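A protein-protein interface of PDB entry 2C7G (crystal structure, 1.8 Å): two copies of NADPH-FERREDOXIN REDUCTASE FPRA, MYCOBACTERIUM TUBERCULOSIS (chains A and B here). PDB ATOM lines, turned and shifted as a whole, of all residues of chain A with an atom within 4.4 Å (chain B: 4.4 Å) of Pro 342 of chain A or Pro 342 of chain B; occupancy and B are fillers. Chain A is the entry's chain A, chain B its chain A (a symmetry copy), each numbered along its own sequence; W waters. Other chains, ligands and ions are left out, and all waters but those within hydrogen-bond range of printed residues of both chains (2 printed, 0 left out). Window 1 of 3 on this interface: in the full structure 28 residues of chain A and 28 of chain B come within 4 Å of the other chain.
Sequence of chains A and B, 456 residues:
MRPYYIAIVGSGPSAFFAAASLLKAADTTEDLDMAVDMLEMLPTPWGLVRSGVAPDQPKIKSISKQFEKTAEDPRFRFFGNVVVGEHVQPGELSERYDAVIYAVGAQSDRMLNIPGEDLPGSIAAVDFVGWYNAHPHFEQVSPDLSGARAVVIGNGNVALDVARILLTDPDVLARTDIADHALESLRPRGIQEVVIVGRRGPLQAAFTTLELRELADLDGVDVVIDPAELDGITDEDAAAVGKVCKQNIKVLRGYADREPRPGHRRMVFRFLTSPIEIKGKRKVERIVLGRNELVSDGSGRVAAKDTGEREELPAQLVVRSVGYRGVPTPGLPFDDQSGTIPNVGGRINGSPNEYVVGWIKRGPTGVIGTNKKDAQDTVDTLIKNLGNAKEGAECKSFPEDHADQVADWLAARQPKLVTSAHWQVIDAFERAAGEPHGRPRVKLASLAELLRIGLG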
ATOM      1  N   PRO A 333      -0.757  21.368  -2.961  1.00  0.00           N
ATOM      2  CA  PRO A 333      -0.384  21.693  -4.348  1.00  0.00           C
ATOM      3  C   PRO A 333      -1.380  21.070  -5.337  1.00  0.00           C
ATOM      4  O   PRO A 333      -2.167  20.177  -4.971  1.00  0.00           O
ATOM      5  CB  PRO A 333       1.002  21.064  -4.505  1.00  0.00           C
ATOM      6  CG  PRO A 333       1.064  19.986  -3.467  1.00  0.00           C
ATOM      7  CD  PRO A 333       0.197  20.431  -2.327  1.00  0.00           C
ATOM      8  N   PHE A 334      -1.332  21.521  -6.584  1.00  0.00           N
ATOM      9  CA  PHE A 334      -2.314  21.085  -7.578  1.00  0.00           C
ATOM     10  C   PHE A 334      -1.774  21.314  -8.990  1.00  0.00           C
ATOM     11  O   PHE A 334      -1.044  22.283  -9.231  1.00  0.00           O
ATOM     12  CB  PHE A 334      -3.630  21.834  -7.350  1.00  0.00           C
ATOM     13  CG  PHE A 334      -4.810  21.267  -8.101  1.00  0.00           C
ATOM     14  CD1 PHE A 334      -5.398  20.055  -7.709  1.00  0.00           C
ATOM     15  CD2 PHE A 334      -5.357  21.968  -9.175  1.00  0.00           C
ATOM     16  CE1 PHE A 334      -6.496  19.549  -8.385  1.00  0.00           C
ATOM     17  CE2 PHE A 334      -6.458  21.460  -9.867  1.00  0.00           C
ATOM     18  CZ  PHE A 334      -7.025  20.247  -9.467  1.00  0.00           C
ATOM     19  N   ASP A 335      -2.093  20.394  -9.897  1.00  0.00           N
ATOM     20  CA  ASP A 335      -1.753  20.540 -11.303  1.00  0.00           C
ATOM     21  C   ASP A 335      -3.030  20.912 -12.049  1.00  0.00           C
ATOM     22  O   ASP A 335      -3.902  20.069 -12.257  1.00  0.00           O
ATOM     23  CB  ASP A 335      -1.152  19.246 -11.871  1.00  0.00           C
ATOM     24  CG  ASP A 335      -0.806  19.361 -13.347  1.00  0.00           C
ATOM     25  OD1 ASP A 335       0.045  20.184 -13.705  1.00  0.00           O
ATOM     26  OD2 ASP A 335      -1.381  18.610 -14.152  1.00  0.00           O
ATOM     27  N   THR A 340      -5.138  17.113 -11.012  1.00  0.00           N
ATOM     28  CA  THR A 340      -4.635  16.130 -10.048  1.00  0.00           C
ATOM     29  C   THR A 340      -3.689  16.785  -9.046  1.00  0.00           C
ATOM     30  O   THR A 340      -3.209  17.896  -9.278  1.00  0.00           O
ATOM     31  CB  THR A 340      -3.893  14.946 -10.736  1.00  0.00           C
ATOM     32  OG1 THR A 340      -2.715  15.429 -11.404  1.00  0.00           O
ATOM     33  CG2 THR A 340      -4.805  14.233 -11.743  1.00  0.00           C
ATOM     34  N   ILE A 341      -3.432  16.101  -7.929  1.00  0.00           N
ATOM     35  CA  ILE A 341      -2.441  16.588  -6.947  1.00  0.00           C
ATOM     36  C   ILE A 341      -1.103  15.920  -7.246  1.00  0.00           C
ATOM     37  O   ILE A 341      -1.031  14.679  -7.267  1.00  0.00           O
ATOM     38  CB  ILE A 341      -2.889  16.279  -5.486  1.00  0.00           C
ATOM     39  CG1 ILE A 341      -4.155  17.067  -5.153  1.00  0.00           C
ATOM     40  CG2 ILE A 341      -1.782  16.618  -4.471  1.00  0.00           C
ATOM     41  CD1 ILE A 341      -4.858  16.611  -3.867  1.00  0.00           C
ATOM     42  N   PRO A 342      -0.039  16.715  -7.487  1.00  0.00           N
ATOM     43  CA  PRO A 342       1.226  16.054  -7.819  1.00  0.00           C
ATOM     44  C   PRO A 342       1.724  15.193  -6.664  1.00  0.00           C
ATOM     45  O   PRO A 342       1.607  15.578  -5.482  1.00  0.00           O
ATOM     46  CB  PRO A 342       2.187  17.223  -8.067  1.00  0.00           C
ATOM     47  CG  PRO A 342       1.627  18.347  -7.251  1.00  0.00           C
ATOM     48  CD  PRO A 342       0.112  18.184  -7.455  1.00  0.00           C
ATOM     49  N   ASN A 343       2.285  14.040  -7.004  1.00  0.00           N
ATOM     50  CA  ASN A 343       2.684  13.069  -6.012  1.00  0.00           C
ATOM     51  C   ASN A 343       3.815  12.168  -6.495  1.00  0.00           C
ATOM     52  O   ASN A 343       4.017  11.966  -7.696  1.00  0.00           O
ATOM     53  CB  ASN A 343       1.479  12.226  -5.593  1.00  0.00           C
ATOM     54  CG  ASN A 343       0.984  11.305  -6.705  1.00  0.00           C
ATOM     55  OD1 ASN A 343       1.365  10.140  -6.763  1.00  0.00           O
ATOM     56  ND2 ASN A 343       0.130  11.826  -7.584  1.00  0.00           N
ATOM     57  N   ILE A 348       2.169  13.122  -1.431  1.00  0.00           N
ATOM     58  CA  ILE A 348       2.035  14.482  -1.967  1.00  0.00           C
ATOM     59  C   ILE A 348       3.369  15.226  -2.087  1.00  0.00           C
ATOM     60  O   ILE A 348       4.157  15.239  -1.160  1.00  0.00           O
ATOM     61  CB  ILE A 348       1.056  15.334  -1.120  1.00  0.00           C
ATOM     62  CG1 ILE A 348      -0.361  14.743  -1.231  1.00  0.00           C
ATOM     63  CG2 ILE A 348       1.098  16.816  -1.572  1.00  0.00           C
ATOM     64  CD1 ILE A 348      -1.496  15.610  -0.701  1.00  0.00           C
ATOM     65  N   ASN A 349       3.596  15.874  -3.227  1.00  0.00           N
ATOM     66  CA  ASN A 349       4.829  16.621  -3.428  1.00  0.00           C
ATOM     67  C   ASN A 349       5.161  17.532  -2.270  1.00  0.00           C
ATOM     68  O   ASN A 349       4.335  18.344  -1.856  1.00  0.00           O
ATOM     69  CB  ASN A 349       4.759  17.476  -4.691  1.00  0.00           C
ATOM     70  CG  ASN A 349       6.076  18.145  -4.989  1.00  0.00           C
ATOM     71  OD1 ASN A 349       6.235  19.354  -4.832  1.00  0.00           O
ATOM     72  ND2 ASN A 349       7.044  17.352  -5.374  1.00  0.00           N
ATOM     73  N   PRO B 333       9.782  23.214  -9.766  1.00  0.00           N
ATOM     74  CA  PRO B 333       9.388  22.586  -8.493  1.00  0.00           C
ATOM     75  C   PRO B 333      10.256  21.352  -8.206  1.00  0.00           C
ATOM     76  O   PRO B 333      10.946  20.835  -9.105  1.00  0.00           O
ATOM     77  CB  PRO B 333       7.930  22.182  -8.726  1.00  0.00           C
ATOM     78  CG  PRO B 333       7.787  22.073 -10.214  1.00  0.00           C
ATOM     79  CD  PRO B 333       8.752  23.051 -10.815  1.00  0.00           C
ATOM     80  N   PHE B 334      10.205  20.871  -6.970  1.00  0.00           N
ATOM     81  CA  PHE B 334      11.082  19.774  -6.556  1.00  0.00           C
ATOM     82  C   PHE B 334      10.509  19.078  -5.321  1.00  0.00           C
ATOM     83  O   PHE B 334       9.891  19.728  -4.468  1.00  0.00           O
ATOM     84  CB  PHE B 334      12.487  20.322  -6.293  1.00  0.00           C
ATOM     85  CG  PHE B 334      13.555  19.265  -6.157  1.00  0.00           C
ATOM     86  CD1 PHE B 334      14.011  18.553  -7.277  1.00  0.00           C
ATOM     87  CD2 PHE B 334      14.133  19.012  -4.913  1.00  0.00           C
ATOM     88  CE1 PHE B 334      15.008  17.599  -7.152  1.00  0.00           C
ATOM     89  CE2 PHE B 334      15.133  18.047  -4.779  1.00  0.00           C
ATOM     90  CZ  PHE B 334      15.567  17.341  -5.904  1.00  0.00           C
ATOM     91  N   ASP B 335      10.674  17.760  -5.260  1.00  0.00           N
ATOM     92  CA  ASP B 335      10.291  16.983  -4.093  1.00  0.00           C
ATOM     93  C   ASP B 335      11.568  16.614  -3.346  1.00  0.00           C
ATOM     94  O   ASP B 335      12.322  15.746  -3.785  1.00  0.00           O
ATOM     95  CB  ASP B 335       9.514  15.720  -4.492  1.00  0.00           C
ATOM     96  CG  ASP B 335       9.117  14.874  -3.292  1.00  0.00           C
ATOM     97  OD1 ASP B 335       8.356  15.352  -2.442  1.00  0.00           O
ATOM     98  OD2 ASP B 335       9.560  13.717  -3.209  1.00  0.00           O
ATOM     99  N   THR B 340      13.249  14.223  -6.724  1.00  0.00           N
ATOM    100  CA  THR B 340      12.676  14.189  -8.072  1.00  0.00           C
ATOM    101  C   THR B 340      11.862  15.449  -8.350  1.00  0.00           C
ATOM    102  O   THR B 340      11.509  16.179  -7.422  1.00  0.00           O
ATOM    103  CB  THR B 340      11.766  12.945  -8.302  1.00  0.00           C
ATOM    104  OG1 THR B 340      10.626  13.006  -7.429  1.00  0.00           O
ATOM    105  CG2 THR B 340      12.540  11.643  -8.057  1.00  0.00           C
ATOM    106  N   ILE B 341      11.575  15.708  -9.628  1.00  0.00           N
ATOM    107  CA  ILE B 341      10.696  16.836  -9.999  1.00  0.00           C
ATOM    108  C   ILE B 341       9.275  16.303 -10.154  1.00  0.00           C
ATOM    109  O   ILE B 341       9.053  15.377 -10.953  1.00  0.00           O
ATOM    110  CB  ILE B 341      11.169  17.515 -11.320  1.00  0.00           C
ATOM    111  CG1 ILE B 341      12.534  18.167 -11.108  1.00  0.00           C
ATOM    112  CG2 ILE B 341      10.158  18.569 -11.808  1.00  0.00           C
ATOM    113  CD1 ILE B 341      13.236  18.592 -12.407  1.00  0.00           C
ATOM    114  N   PRO B 342       8.305  16.863  -9.400  1.00  0.00           N
ATOM    115  CA  PRO B 342       6.955  16.305  -9.530  1.00  0.00           C
ATOM    116  C   PRO B 342       6.411  16.487 -10.941  1.00  0.00           C
ATOM    117  O   PRO B 342       6.626  17.539 -11.580  1.00  0.00           O
ATOM    118  CB  PRO B 342       6.131  17.126  -8.529  1.00  0.00           C
ATOM    119  CG  PRO B 342       6.860  18.431  -8.426  1.00  0.00           C
ATOM    120  CD  PRO B 342       8.333  17.993  -8.450  1.00  0.00           C
ATOM    121  N   ASN B 343       5.700  15.474 -11.421  1.00  0.00           N
ATOM    122  CA  ASN B 343       5.232  15.455 -12.787  1.00  0.00           C
ATOM    123  C   ASN B 343       3.981  14.604 -12.967  1.00  0.00           C
ATOM    124  O   ASN B 343       3.702  13.686 -12.189  1.00  0.00           O
ATOM    125  CB  ASN B 343       6.345  14.960 -13.712  1.00  0.00           C
ATOM    126  CG  ASN B 343       6.675  13.484 -13.507  1.00  0.00           C
ATOM    127  OD1 ASN B 343       6.155  12.627 -14.213  1.00  0.00           O
ATOM    128  ND2 ASN B 343       7.545  13.189 -12.542  1.00  0.00           N
ATOM    129  N   ILE B 348       5.958  18.451 -16.215  1.00  0.00           N
ATOM    130  CA  ILE B 348       6.230  19.092 -14.922  1.00  0.00           C
ATOM    131  C   ILE B 348       4.991  19.726 -14.281  1.00  0.00           C
ATOM    132  O   ILE B 348       4.253  20.441 -14.933  1.00  0.00           O
ATOM    133  CB  ILE B 348       7.343  20.165 -15.041  1.00  0.00           C
ATOM    134  CG1 ILE B 348       8.671  19.483 -15.412  1.00  0.00           C
ATOM    135  CG2 ILE B 348       7.458  20.972 -13.724  1.00  0.00           C
ATOM    136  CD1 ILE B 348       9.925  20.339 -15.290  1.00  0.00           C
ATOM    137  N   ASN B 349       4.793  19.483 -12.988  1.00  0.00           N
ATOM    138  CA  ASN B 349       3.650  20.053 -12.289  1.00  0.00           C
ATOM    139  C   ASN B 349       3.483  21.533 -12.543  1.00  0.00           C
ATOM    140  O   ASN B 349       4.419  22.309 -12.356  1.00  0.00           O
ATOM    141  CB  ASN B 349       3.765  19.847 -10.780  1.00  0.00           C
ATOM    142  CG  ASN B 349       2.526  20.306 -10.056  1.00  0.00           C
ATOM    143  OD1 ASN B 349       2.521  21.326  -9.370  1.00  0.00           O
ATOM    144  ND2 ASN B 349       1.453  19.580 -10.245  1.00  0.00           N
HETATM  145  O   HOH W   1       2.076  13.408  -9.947  1.00  0.00           O
HETATM  146  O   HOH W   2       5.697  13.041  -9.636  1.00  0.00           O
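N of Asp 335 of chain A lies within hydrogen-bond range of O of Thr 340 of chain A.
O of Pro 342 of chain A lies within hydrogen-bond range of N of Asn 349 of chain A, at 3.0 Å.
The backbone carbonyl oxygen of Thr 340 of chain B is in hydrogen-bond range of the backbone NH of Asp 335 of chain B, 2.8 Å away.
The backbone NH (N) of Asn 349 of chain B sits at hydrogen-bond distance from the backbone carbonyl oxygen (O) of Pro 342 of chain B (3.0 Å).
Along chain A the printed residues that touch a printed residue of chain B span positions 334 to 349.
Of the 9 printed residues of chain B, 4 touch a printed residue of chain A.
Among the printed residues, 7 pairs touch across the chains.
O of Phe 334 of chain A touches OD1 of Asn 349 of chain B (3.7 Å).
Asp 335 of chain A touches Asn 349 of chain B (CB to ND2, 3.1 Å).
Pro 342 of chain B touches Pro 342 of chain A.
Asn 349 of chain B touches Pro 342 of chain A.
Asn 349 of chain A touches Phe 334 of chain B.
ND2 of Asn 349 of chain A touches CB of Asp 335 of chain B, at 3.1 Å.
Asn 349 of chain A touches Pro 342 of chain B.
Of the printed residues of chain B, Phe 334 of chain A touches Asn 349.
Pro 342 of chain A touches just these residues of chain B: Pro 342 and Asn 349.
Printed residues of chain B within 4 Å of Asn 349 of chain A: Phe 334 (3.7 Å), Asp 335 (3.1 Å) and Pro 342 (3.2 Å).
Of the printed residues of chain A, Phe 334 of chain B touches Asn 349 (3.7 Å).
Of the printed residues of chain A, Asp 335 of chain B touches Asn 349 (3.1 Å).
Printed residues of chain A within 4 Å of Asn 349 of chain B: Phe 334, Asp 335 and Pro 342.
The nearest printed residue of chain B that does not touch Pro 342 of chain A is Asn 343 of chain B (5.2 Å).
Water W2 bridges O of Asn 343 of chain A and N of Asn 343 of chain B.
Water W1 bridges the backbone carbonyl oxygen of Asn 343 of chain B (2.8 Å) and the backbone NH of Asn 343 of chain A (3.0 Å).
Phe 334 of chain A touches Asn 349 of chain B, and with the chains exchanged Asn 349 of chain A touches Phe 334 of chain B.
Asp 335 of chain A touches Asn 349 of chain B, and with the chains exchanged Asn 349 of chain A touches Asp 335 of chain B.
Pro 342 of chain B touches its own counterpart, Pro 342 of chain A.
Pro 342 of chain A touches Asn 349 of chain B, and with the chains exchanged Asn 349 of chain A touches Pro 342 of chain B.
9 positions are printed for both chains.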
